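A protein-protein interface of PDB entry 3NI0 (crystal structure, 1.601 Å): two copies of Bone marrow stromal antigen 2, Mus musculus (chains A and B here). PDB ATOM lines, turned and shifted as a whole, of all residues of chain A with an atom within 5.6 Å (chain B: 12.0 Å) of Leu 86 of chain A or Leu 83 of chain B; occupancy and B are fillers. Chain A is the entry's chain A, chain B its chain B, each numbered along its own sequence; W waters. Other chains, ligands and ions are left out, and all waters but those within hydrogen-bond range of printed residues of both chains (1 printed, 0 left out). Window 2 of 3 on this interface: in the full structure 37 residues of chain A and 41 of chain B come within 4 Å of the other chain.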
ATOM      1  N   LEU A  79      18.457  13.093   4.524  1.00  0.00           N
ATOM      2  CA  LEU A  79      19.864  13.130   4.145  1.00  0.00           C
ATOM      3  C   LEU A  79      20.025  13.492   2.670  1.00  0.00           C
ATOM      4  O   LEU A  79      20.958  14.202   2.297  1.00  0.00           O
ATOM      5  CB  LEU A  79      20.531  11.785   4.439  1.00  0.00           C
ATOM      6  CG  LEU A  79      20.541  11.384   5.917  1.00  0.00           C
ATOM      7  CD1 LEU A  79      21.075   9.968   6.091  1.00  0.00           C
ATOM      8  CD2 LEU A  79      21.358  12.373   6.733  1.00  0.00           C
ATOM      9  N   GLN A  81      18.052  15.425   1.065  1.00  0.00           N
ATOM     10  CA  GLN A  81      17.756  16.846   0.952  1.00  0.00           C
ATOM     11  C   GLN A  81      18.955  17.672   1.402  1.00  0.00           C
ATOM     12  O   GLN A  81      19.191  18.760   0.883  1.00  0.00           O
ATOM     13  CB  GLN A  81      16.517  17.222   1.765  1.00  0.00           C
ATOM     14  CG  GLN A  81      15.998  18.624   1.464  1.00  0.00           C
ATOM     15  CD  GLN A  81      15.813  18.872  -0.023  1.00  0.00           C
ATOM     16  OE1 GLN A  81      16.351  19.833  -0.578  1.00  0.00           O
ATOM     17  NE2 GLN A  81      15.047  18.005  -0.678  1.00  0.00           N
ATOM     18  N   GLU A  82      19.709  17.155   2.367  1.00  0.00           N
ATOM     19  CA  GLU A  82      20.911  17.840   2.838  1.00  0.00           C
ATOM     20  C   GLU A  82      21.990  17.830   1.759  1.00  0.00           C
ATOM     21  O   GLU A  82      22.683  18.826   1.555  1.00  0.00           O
ATOM     22  CB  GLU A  82      21.436  17.194   4.122  1.00  0.00           C
ATOM     23  CG  GLU A  82      20.504  17.347   5.312  1.00  0.00           C
ATOM     24  CD  GLU A  82      21.050  16.709   6.576  1.00  0.00           C
ATOM     25  OE1 GLU A  82      22.236  16.320   6.584  1.00  0.00           O
ATOM     26  OE2 GLU A  82      20.292  16.604   7.562  1.00  0.00           O
ATOM     27  N   LEU A  83      22.123  16.703   1.067  1.00  0.00           N
ATOM     28  CA  LEU A  83      23.074  16.585  -0.031  1.00  0.00           C
ATOM     29  C   LEU A  83      22.655  17.484  -1.179  1.00  0.00           C
ATOM     30  O   LEU A  83      23.487  18.134  -1.808  1.00  0.00           O
ATOM     31  CB  LEU A  83      23.150  15.138  -0.512  1.00  0.00           C
ATOM     32  CG  LEU A  83      23.917  14.197   0.413  1.00  0.00           C
ATOM     33  CD1 LEU A  83      23.612  12.744   0.074  1.00  0.00           C
ATOM     34  CD2 LEU A  83      25.408  14.478   0.329  1.00  0.00           C
ATOM     35  N   GLU A  84      21.354  17.520  -1.442  1.00  0.00           N
ATOM     36  CA  GLU A  84      20.816  18.335  -2.516  1.00  0.00           C
ATOM     37  C   GLU A  84      21.054  19.807  -2.221  1.00  0.00           C
ATOM     38  O   GLU A  84      21.325  20.590  -3.128  1.00  0.00           O
ATOM     39  CB  GLU A  84      19.320  18.083  -2.679  1.00  0.00           C
ATOM     40  CG  GLU A  84      18.763  18.640  -3.969  1.00  0.00           C
ATOM     41  CD  GLU A  84      19.189  17.831  -5.176  1.00  0.00           C
ATOM     42  OE1 GLU A  84      19.970  16.872  -5.007  1.00  0.00           O
ATOM     43  OE2 GLU A  84      18.728  18.137  -6.292  1.00  0.00           O
ATOM     44  N   ASN A  85      20.953  20.177  -0.948  1.00  0.00           N
ATOM     45  CA  ASN A  85      21.171  21.559  -0.539  1.00  0.00           C
ATOM     46  C   ASN A  85      22.613  21.982  -0.783  1.00  0.00           C
ATOM     47  O   ASN A  85      22.865  23.106  -1.209  1.00  0.00           O
ATOM     48  CB  ASN A  85      20.810  21.758   0.936  1.00  0.00           C
ATOM     49  CG  ASN A  85      19.325  21.557   1.215  1.00  0.00           C
ATOM     50  OD1 ASN A  85      18.927  21.316   2.356  1.00  0.00           O
ATOM     51  ND2 ASN A  85      18.503  21.641   0.172  1.00  0.00           N
ATOM     52  N   LEU A  86      23.556  21.086  -0.507  1.00  0.00           N
ATOM     53  CA  LEU A  86      24.966  21.370  -0.763  1.00  0.00           C
ATOM     54  C   LEU A  86      25.208  21.539  -2.259  1.00  0.00           C
ATOM     55  O   LEU A  86      25.979  22.403  -2.673  1.00  0.00           O
ATOM     56  CB  LEU A  86      25.861  20.255  -0.216  1.00  0.00           C
ATOM     57  CG  LEU A  86      26.004  20.158   1.305  1.00  0.00           C
ATOM     58  CD1 LEU A  86      26.674  18.847   1.685  1.00  0.00           C
ATOM     59  CD2 LEU A  86      26.782  21.341   1.861  1.00  0.00           C
ATOM     60  N   ARG A  87      24.546  20.716  -3.068  1.00  0.00           N
ATOM     61  CA  ARG A  87      24.694  20.796  -4.518  1.00  0.00           C
ATOM     62  C   ARG A  87      24.136  22.111  -5.040  1.00  0.00           C
ATOM     63  O   ARG A  87      24.696  22.710  -5.954  1.00  0.00           O
ATOM     64  CB  ARG A  87      23.982  19.632  -5.210  1.00  0.00           C
ATOM     65  CG  ARG A  87      24.627  18.281  -4.972  1.00  0.00           C
ATOM     66  CD  ARG A  87      24.027  17.218  -5.873  1.00  0.00           C
ATOM     67  NE  ARG A  87      24.422  15.872  -5.465  1.00  0.00           N
ATOM     68  CZ  ARG A  87      23.602  14.981  -4.912  1.00  0.00           C
ATOM     69  NH1 ARG A  87      22.327  15.280  -4.703  1.00  0.00           N
ATOM     70  NH2 ARG A  87      24.057  13.782  -4.570  1.00  0.00           N
ATOM     71  N   ILE A  88      23.031  22.559  -4.456  1.00  0.00           N
ATOM     72  CA  ILE A  88      22.412  23.810  -4.870  1.00  0.00           C
ATOM     73  C   ILE A  88      23.272  24.996  -4.456  1.00  0.00           C
ATOM     74  O   ILE A  88      23.364  25.977  -5.186  1.00  0.00           O
ATOM     75  CB  ILE A  88      21.001  23.962  -4.283  1.00  0.00           C
ATOM     76  CG1 ILE A  88      20.050  22.966  -4.944  1.00  0.00           C
ATOM     77  CG2 ILE A  88      20.480  25.375  -4.494  1.00  0.00           C
ATOM     78  CD1 ILE A  88      18.656  22.978  -4.357  1.00  0.00           C
ATOM     79  N   GLN A  89      23.906  24.907  -3.290  1.00  0.00           N
ATOM     80  CA  GLN A  89      24.791  25.979  -2.833  1.00  0.00           C
ATOM     81  C   GLN A  89      25.970  26.145  -3.791  1.00  0.00           C
ATOM     82  O   GLN A  89      26.408  27.263  -4.054  1.00  0.00           O
ATOM     83  CB  GLN A  89      25.281  25.720  -1.405  1.00  0.00           C
ATOM     84  CG  GLN A  89      24.221  25.986  -0.338  1.00  0.00           C
ATOM     85  CD  GLN A  89      24.709  25.697   1.073  1.00  0.00           C
ATOM     86  OE1 GLN A  89      25.729  26.229   1.511  1.00  0.00           O
ATOM     87  NE2 GLN A  89      23.976  24.852   1.791  1.00  0.00           N
ATOM     88  N   LYS A  90      26.476  25.033  -4.314  1.00  0.00           N
ATOM     89  CA  LYS A  90      27.548  25.079  -5.306  1.00  0.00           C
ATOM     90  C   LYS A  90      27.028  25.661  -6.615  1.00  0.00           C
ATOM     91  O   LYS A  90      27.666  26.518  -7.229  1.00  0.00           O
ATOM     92  CB  LYS A  90      28.114  23.679  -5.551  1.00  0.00           C
ATOM     93  CG  LYS A  90      29.185  23.634  -6.633  1.00  0.00           C
ATOM     94  CD  LYS A  90      29.711  22.222  -6.844  1.00  0.00           C
ATOM     95  CE  LYS A  90      30.533  22.116  -8.122  1.00  0.00           C
ATOM     96  NZ  LYS A  90      31.785  22.922  -8.064  1.00  0.00           N
ATOM     97  N   GLU A  91      25.862  25.185  -7.032  1.00  0.00           N
ATOM     98  CA  GLU A  91      25.214  25.649  -8.250  1.00  0.00           C
ATOM     99  C   GLU A  91      25.062  27.167  -8.262  1.00  0.00           C
ATOM    100  O   GLU A  91      25.204  27.808  -9.303  1.00  0.00           O
ATOM    101  CB  GLU A  91      23.834  25.002  -8.368  1.00  0.00           C
ATOM    102  CG  GLU A  91      23.006  25.485  -9.538  1.00  0.00           C
ATOM    103  CD  GLU A  91      21.539  25.142  -9.383  1.00  0.00           C
ATOM    104  OE1 GLU A  91      21.229  23.982  -9.039  1.00  0.00           O
ATOM    105  OE2 GLU A  91      20.696  26.036  -9.588  1.00  0.00           O
ATOM    106  N   ASN B  74      21.608   0.555   5.016  1.00  0.00           N
ATOM    107  CA  ASN B  74      22.806   0.698   4.201  1.00  0.00           C
ATOM    108  C   ASN B  74      22.824   2.042   3.484  1.00  0.00           C
ATOM    109  O   ASN B  74      23.875   2.670   3.355  1.00  0.00           O
ATOM    110  CB  ASN B  74      22.901  -0.438   3.184  1.00  0.00           C
ATOM    111  CG  ASN B  74      23.281  -1.761   3.820  1.00  0.00           C
ATOM    112  OD1 ASN B  74      23.898  -1.796   4.885  1.00  0.00           O
ATOM    113  ND2 ASN B  74      22.925  -2.859   3.163  1.00  0.00           N
ATOM    114  N   GLU B  75      21.660   2.481   3.017  1.00  0.00           N
ATOM    115  CA  GLU B  75      21.555   3.756   2.318  1.00  0.00           C
ATOM    116  C   GLU B  75      21.806   4.909   3.274  1.00  0.00           C
ATOM    117  O   GLU B  75      22.451   5.892   2.918  1.00  0.00           O
ATOM    118  CB  GLU B  75      20.179   3.923   1.676  1.00  0.00           C
ATOM    119  CG  GLU B  75      20.072   5.156   0.797  1.00  0.00           C
ATOM    120  CD  GLU B  75      20.896   5.044  -0.474  1.00  0.00           C
ATOM    121  OE1 GLU B  75      21.476   3.965  -0.716  1.00  0.00           O
ATOM    122  OE2 GLU B  75      20.961   6.037  -1.229  1.00  0.00           O
ATOM    123  N   VAL B  76      21.287   4.793   4.487  1.00  0.00           N
ATOM    124  CA  VAL B  76      21.475   5.838   5.475  1.00  0.00           C
ATOM    125  C   VAL B  76      22.956   6.006   5.805  1.00  0.00           C
ATOM    126  O   VAL B  76      23.460   7.126   5.876  1.00  0.00           O
ATOM    127  CB  VAL B  76      20.726   5.528   6.766  1.00  0.00           C
ATOM    128  CG1 VAL B  76      21.239   6.399   7.864  1.00  0.00           C
ATOM    129  CG2 VAL B  76      19.215   5.697   6.577  1.00  0.00           C
ATOM    130  N   THR B  77      23.643   4.890   6.025  1.00  0.00           N
ATOM    131  CA  THR B  77      25.067   4.919   6.343  1.00  0.00           C
ATOM    132  C   THR B  77      25.848   5.524   5.181  1.00  0.00           C
ATOM    133  O   THR B  77      26.751   6.333   5.380  1.00  0.00           O
ATOM    134  CB  THR B  77      25.611   3.505   6.627  1.00  0.00           C
ATOM    135  OG1 THR B  77      24.869   2.902   7.695  1.00  0.00           O
ATOM    136  CG2 THR B  77      27.083   3.565   7.009  1.00  0.00           C
ATOM    137  N   LYS B  78      25.486   5.121   3.969  1.00  0.00           N
ATOM    138  CA  LYS B  78      26.143   5.602   2.760  1.00  0.00           C
ATOM    139  C   LYS B  78      26.015   7.118   2.635  1.00  0.00           C
ATOM    140  O   LYS B  78      27.008   7.820   2.450  1.00  0.00           O
ATOM    141  CB  LYS B  78      25.525   4.926   1.535  1.00  0.00           C
ATOM    142  CG  LYS B  78      26.361   5.014   0.272  1.00  0.00           C
ATOM    143  CD  LYS B  78      25.830   4.067  -0.794  1.00  0.00           C
ATOM    144  CE  LYS B  78      25.068   4.806  -1.883  1.00  0.00           C
ATOM    145  NZ  LYS B  78      24.025   5.714  -1.334  1.00  0.00           N
ATOM    146  N   LEU B  79      24.788   7.617   2.742  1.00  0.00           N
ATOM    147  CA  LEU B  79      24.520   9.044   2.607  1.00  0.00           C
ATOM    148  C   LEU B  79      25.187   9.837   3.724  1.00  0.00           C
ATOM    149  O   LEU B  79      25.646  10.959   3.513  1.00  0.00           O
ATOM    150  CB  LEU B  79      23.013   9.307   2.621  1.00  0.00           C
ATOM    151  CG  LEU B  79      22.226   8.724   1.445  1.00  0.00           C
ATOM    152  CD1 LEU B  79      20.733   8.951   1.634  1.00  0.00           C
ATOM    153  CD2 LEU B  79      22.703   9.330   0.137  1.00  0.00           C
ATOM    154  N   ASN B  80      25.234   9.253   4.915  1.00  0.00           N
ATOM    155  CA  ASN B  80      25.827   9.923   6.064  1.00  0.00           C
ATOM    156  C   ASN B  80      27.318  10.137   5.852  1.00  0.00           C
ATOM    157  O   ASN B  80      27.855  11.200   6.162  1.00  0.00           O
ATOM    158  CB  ASN B  80      25.582   9.109   7.333  1.00  0.00           C
ATOM    159  CG  ASN B  80      25.348   9.981   8.545  1.00  0.00           C
ATOM    160  OD1 ASN B  80      24.289  10.592   8.690  1.00  0.00           O
ATOM    161  ND2 ASN B  80      26.334  10.038   9.430  1.00  0.00           N
ATOM    162  N   GLN B  81      27.979   9.119   5.312  1.00  0.00           N
ATOM    163  CA  GLN B  81      29.408   9.188   5.029  1.00  0.00           C
ATOM    164  C   GLN B  81      29.688  10.180   3.908  1.00  0.00           C
ATOM    165  O   GLN B  81      30.659  10.929   3.966  1.00  0.00           O
ATOM    166  CB  GLN B  81      29.945   7.812   4.636  1.00  0.00           C
ATOM    167  CG  GLN B  81      29.887   6.778   5.744  1.00  0.00           C
ATOM    168  CD  GLN B  81      30.215   5.383   5.251  1.00  0.00           C
ATOM    169  OE1 GLN B  81      29.954   5.044   4.096  1.00  0.00           O
ATOM    170  NE2 GLN B  81      30.797   4.568   6.122  1.00  0.00           N
ATOM    171  N   GLU B  82      28.839  10.176   2.885  1.00  0.00           N
ATOM    172  CA  GLU B  82      28.977  11.116   1.779  1.00  0.00           C
ATOM    173  C   GLU B  82      28.903  12.542   2.307  1.00  0.00           C
ATOM    174  O   GLU B  82      29.684  13.410   1.916  1.00  0.00           O
ATOM    175  CB  GLU B  82      27.877  10.890   0.741  1.00  0.00           C
ATOM    176  CG  GLU B  82      28.061   9.649  -0.112  1.00  0.00           C
ATOM    177  CD  GLU B  82      26.912   9.433  -1.081  1.00  0.00           C
ATOM    178  OE1 GLU B  82      26.166  10.397  -1.353  1.00  0.00           O
ATOM    179  OE2 GLU B  82      26.758   8.296  -1.574  1.00  0.00           O
ATOM    180  N   LEU B  83      27.953  12.775   3.204  1.00  0.00           N
ATOM    181  CA  LEU B  83      27.751  14.092   3.788  1.00  0.00           C
ATOM    182  C   LEU B  83      28.927  14.511   4.658  1.00  0.00           C
ATOM    183  O   LEU B  83      29.307  15.682   4.676  1.00  0.00           O
ATOM    184  CB  LEU B  83      26.466  14.109   4.610  1.00  0.00           C
ATOM    185  CG  LEU B  83      25.213  14.463   3.814  1.00  0.00           C
ATOM    186  CD1 LEU B  83      23.953  14.082   4.573  1.00  0.00           C
ATOM    187  CD2 LEU B  83      25.225  15.949   3.474  1.00  0.00           C
ATOM    188  N   GLU B  84      29.509  13.556   5.373  1.00  0.00           N
ATOM    189  CA  GLU B  84      30.639  13.858   6.242  1.00  0.00           C
ATOM    190  C   GLU B  84      31.881  14.198   5.427  1.00  0.00           C
ATOM    191  O   GLU B  84      32.594  15.141   5.750  1.00  0.00           O
ATOM    192  CB  GLU B  84      30.941  12.696   7.183  1.00  0.00           C
ATOM    193  CG  GLU B  84      32.286  12.834   7.881  1.00  0.00           C
ATOM    194  CD  GLU B  84      32.261  12.332   9.307  1.00  0.00           C
ATOM    195  OE1 GLU B  84      31.397  11.490   9.626  1.00  0.00           O
ATOM    196  OE2 GLU B  84      33.101  12.789  10.112  1.00  0.00           O
ATOM    197  N   ASN B  85      32.139  13.424   4.378  1.00  0.00           N
ATOM    198  CA  ASN B  85      33.262  13.701   3.490  1.00  0.00           C
ATOM    199  C   ASN B  85      33.140  15.078   2.861  1.00  0.00           C
ATOM    200  O   ASN B  85      34.108  15.831   2.803  1.00  0.00           O
ATOM    201  CB  ASN B  85      33.355  12.645   2.391  1.00  0.00           C
ATOM    202  CG  ASN B  85      34.078  11.395   2.844  1.00  0.00           C
ATOM    203  OD1 ASN B  85      35.173  11.464   3.404  1.00  0.00           O
ATOM    204  ND2 ASN B  85      33.467  10.242   2.609  1.00  0.00           N
ATOM    205  N   LEU B  86      31.941  15.405   2.393  1.00  0.00           N
ATOM    206  CA  LEU B  86      31.717  16.675   1.715  1.00  0.00           C
ATOM    207  C   LEU B  86      31.840  17.845   2.681  1.00  0.00           C
ATOM    208  O   LEU B  86      32.315  18.909   2.304  1.00  0.00           O
ATOM    209  CB  LEU B  86      30.343  16.695   1.041  1.00  0.00           C
ATOM    210  CG  LEU B  86      30.180  15.760  -0.158  1.00  0.00           C
ATOM    211  CD1 LEU B  86      28.727  15.697  -0.596  1.00  0.00           C
ATOM    212  CD2 LEU B  86      31.075  16.205  -1.308  1.00  0.00           C
ATOM    213  N   ARG B  87      31.424  17.647   3.928  1.00  0.00           N
ATOM    214  CA  ARG B  87      31.460  18.724   4.913  1.00  0.00           C
ATOM    215  C   ARG B  87      32.876  18.999   5.411  1.00  0.00           C
ATOM    216  O   ARG B  87      33.258  20.153   5.597  1.00  0.00           O
ATOM    217  CB  ARG B  87      30.510  18.426   6.074  1.00  0.00           C
ATOM    218  CG  ARG B  87      29.084  18.862   5.773  1.00  0.00           C
ATOM    219  CD  ARG B  87      28.061  18.300   6.745  1.00  0.00           C
ATOM    220  NE  ARG B  87      26.710  18.662   6.328  1.00  0.00           N
ATOM    221  CZ  ARG B  87      25.601  18.052   6.736  1.00  0.00           C
ATOM    222  NH1 ARG B  87      25.665  17.033   7.582  1.00  0.00           N
ATOM    223  NH2 ARG B  87      24.422  18.461   6.287  1.00  0.00           N
ATOM    224  N   ILE B  88      33.659  17.944   5.614  1.00  0.00           N
ATOM    225  CA  ILE B  88      35.062  18.112   5.969  1.00  0.00           C
ATOM    226  C   ILE B  88      35.793  18.810   4.831  1.00  0.00           C
ATOM    227  O   ILE B  88      36.580  19.723   5.062  1.00  0.00           O
ATOM    228  CB  ILE B  88      35.749  16.767   6.264  1.00  0.00           C
ATOM    229  CG1 ILE B  88      35.209  16.173   7.565  1.00  0.00           C
ATOM    230  CG2 ILE B  88      37.258  16.957   6.370  1.00  0.00           C
ATOM    231  CD1 ILE B  88      35.679  14.759   7.839  1.00  0.00           C
ATOM    232  N   GLN B  89      35.522  18.385   3.601  1.00  0.00           N
ATOM    233  CA  GLN B  89      36.166  18.974   2.432  1.00  0.00           C
ATOM    234  C   GLN B  89      35.875  20.469   2.336  1.00  0.00           C
ATOM    235  O   GLN B  89      36.766  21.261   2.027  1.00  0.00           O
ATOM    236  CB  GLN B  89      35.721  18.263   1.155  1.00  0.00           C
ATOM    237  CG  GLN B  89      36.308  16.868   0.999  1.00  0.00           C
ATOM    238  CD  GLN B  89      35.739  16.120  -0.187  1.00  0.00           C
ATOM    239  OE1 GLN B  89      35.216  16.722  -1.125  1.00  0.00           O
ATOM    240  NE2 GLN B  89      35.834  14.798  -0.149  1.00  0.00           N
ATOM    241  N   LYS B  90      34.631  20.856   2.595  1.00  0.00           N
ATOM    242  CA  LYS B  90      34.273  22.271   2.594  1.00  0.00           C
ATOM    243  C   LYS B  90      35.031  22.980   3.715  1.00  0.00           C
ATOM    244  O   LYS B  90      35.036  22.534   4.862  1.00  0.00           O
ATOM    245  CB  LYS B  90      32.764  22.475   2.768  1.00  0.00           C
ATOM    246  CG  LYS B  90      31.892  21.796   1.715  1.00  0.00           C
ATOM    247  CD  LYS B  90      32.162  22.295   0.305  1.00  0.00           C
ATOM    248  CE  LYS B  90      31.241  21.607  -0.697  1.00  0.00           C
ATOM    249  NZ  LYS B  90      31.650  21.843  -2.108  1.00  0.00           N
ATOM    250  N   GLU B  91      35.671  24.087   3.360  1.00  0.00           N
ATOM    251  CA  GLU B  91      36.494  24.872   4.282  1.00  0.00           C
ATOM    252  C   GLU B  91      37.428  24.065   5.192  1.00  0.00           C
ATOM    253  O   GLU B  91      37.569  24.368   6.377  1.00  0.00           O
ATOM    254  CB  GLU B  91      35.630  25.826   5.110  1.00  0.00           C
ATOM    255  CG  GLU B  91      34.986  26.924   4.275  1.00  0.00           C
ATOM    256  CD  GLU B  91      34.441  28.061   5.115  1.00  0.00           C
ATOM    257  OE1 GLU B  91      35.057  28.385   6.153  1.00  0.00           O
ATOM    258  OE2 GLU B  91      33.397  28.635   4.737  1.00  0.00           O
ATOM    259  N   THR B  92      38.049  23.030   4.634  1.00  0.00           N
ATOM    260  CA  THR B  92      39.348  22.581   5.122  1.00  0.00           C
ATOM    261  C   THR B  92      40.331  22.807   3.983  1.00  0.00           C
ATOM    262  O   THR B  92      40.001  22.568   2.820  1.00  0.00           O
ATOM    263  CB  THR B  92      39.390  21.093   5.539  1.00  0.00           C
ATOM    264  OG1 THR B  92      38.942  20.269   4.457  1.00  0.00           O
ATOM    265  CG2 THR B  92      38.537  20.842   6.778  1.00  0.00           C
HETATM  266  O   HOH W   1      23.058  20.366   3.784  1.00  0.00           O
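Printed residues of chain A that touch a printed residue of chain B: Leu 79, Glu 82, Leu 83 and Leu 86. Printed residues of chain B that touch a printed residue of chain A: Val 76, Leu 79, Asn 80, Glu 82, Leu 83, Leu 86 and Arg 87. Hydrophobic or aromatic side chains of chain B within 4 Å of the printed part of chain A: Val 76, Leu 79, Leu 83 and Leu 86. Among the printed residues, 11 pairs touch across the chains.
Leu 83 of chain A touches four residues of chain B. Asn 85 of chain A touches none of the printed residues of chain B. Of the printed residues of chain B, Leu 86 of chain A touches Leu 83 (3.7 Å). No residue of chain B comes within 4 Å of Gln 89 of chain A. No residue of chain B comes within 4 Å of Lys 90 of chain A. Of the printed residues of chain A, Val 76 of chain B touches Leu 79 (3.7 Å). Of the printed residues of chain A, Leu 79 of chain B touches Leu 79 (3.95 Å) and Leu 83 (3.5 Å). Of the printed residues of chain A, Asn 80 of chain B touches Leu 79 (3.9 Å). Gln 81 of chain B touches none of the printed residues of chain A. Printed residues of chain A within 4 Å of Leu 86 of chain B: Leu 83. Gln 89 of chain B touches none of the printed residues of chain A. The nearest printed residue of chain A that does not touch Leu 83 of chain B is Glu 84 of chain A (6.5 Å). The nearest printed residue of chain A that does not touch Val 76 of chain B is Leu 83 of chain A (8.1 Å).
The side-chain carboxylate (OE1) of Glu 82 of chain A is in salt-bridge range of the guanidinium group (NH2) of Arg 87 of chain B (3.1 Å).
Glu 82 of chain A touches Leu 83 of chain B, and with the chains exchanged Leu 83 of chain A touches Glu 82 of chain B. Glu 82 of chain A touches Arg 87 of chain B, but with the chains exchanged Arg 87 of chain A does not touch Glu 82 of chain B (5.1 Å). Leu 83 of chain A touches its own counterpart, Leu 83 of chain B. Leu 83 of chain A touches Leu 86 of chain B, and with the chains exchanged Leu 86 of chain A touches Leu 83 of chain B. Of the 11 pairs that touch across the chains among the printed residues, 8 have their exchanged pair printed and touching as well.
OE2 of Glu 82 of chain B lies within salt-bridge range of NZ of Lys 78 of chain B, at 3.8 Å.
Water W1 lies within hydrogen-bond range of the backbone carbonyl oxygen of Glu 82 of chain A and the guanidinium group of Arg 87 of chain B.
Leu 79 of chain A touches Val 76 of chain B (CD1 to O, 3.7 Å). Leu 79 of chain B touches Leu 79 of chain A. CD2 of Leu 79 of chain A touches OD1 of Asn 80 of chain B, 3.9 Å away. O of Leu 79 of chain A touches CD1 of Leu 83 of chain B (3.8 Å). Glu 82 of chain A touches Leu 83 of chain B. CD2 of Leu 79 of chain B touches CD1 of Leu 83 of chain A, 3.5 Å away. Glu 82 of chain B touches Leu 83 of chain A. Leu 83 of chain A touches Leu 83 of chain B. CD1 of Leu 86 of chain B touches CD2 of Leu 83 of chain A, at 3.7 Å. Leu 83 of chain B touches Leu 86 of chain A.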
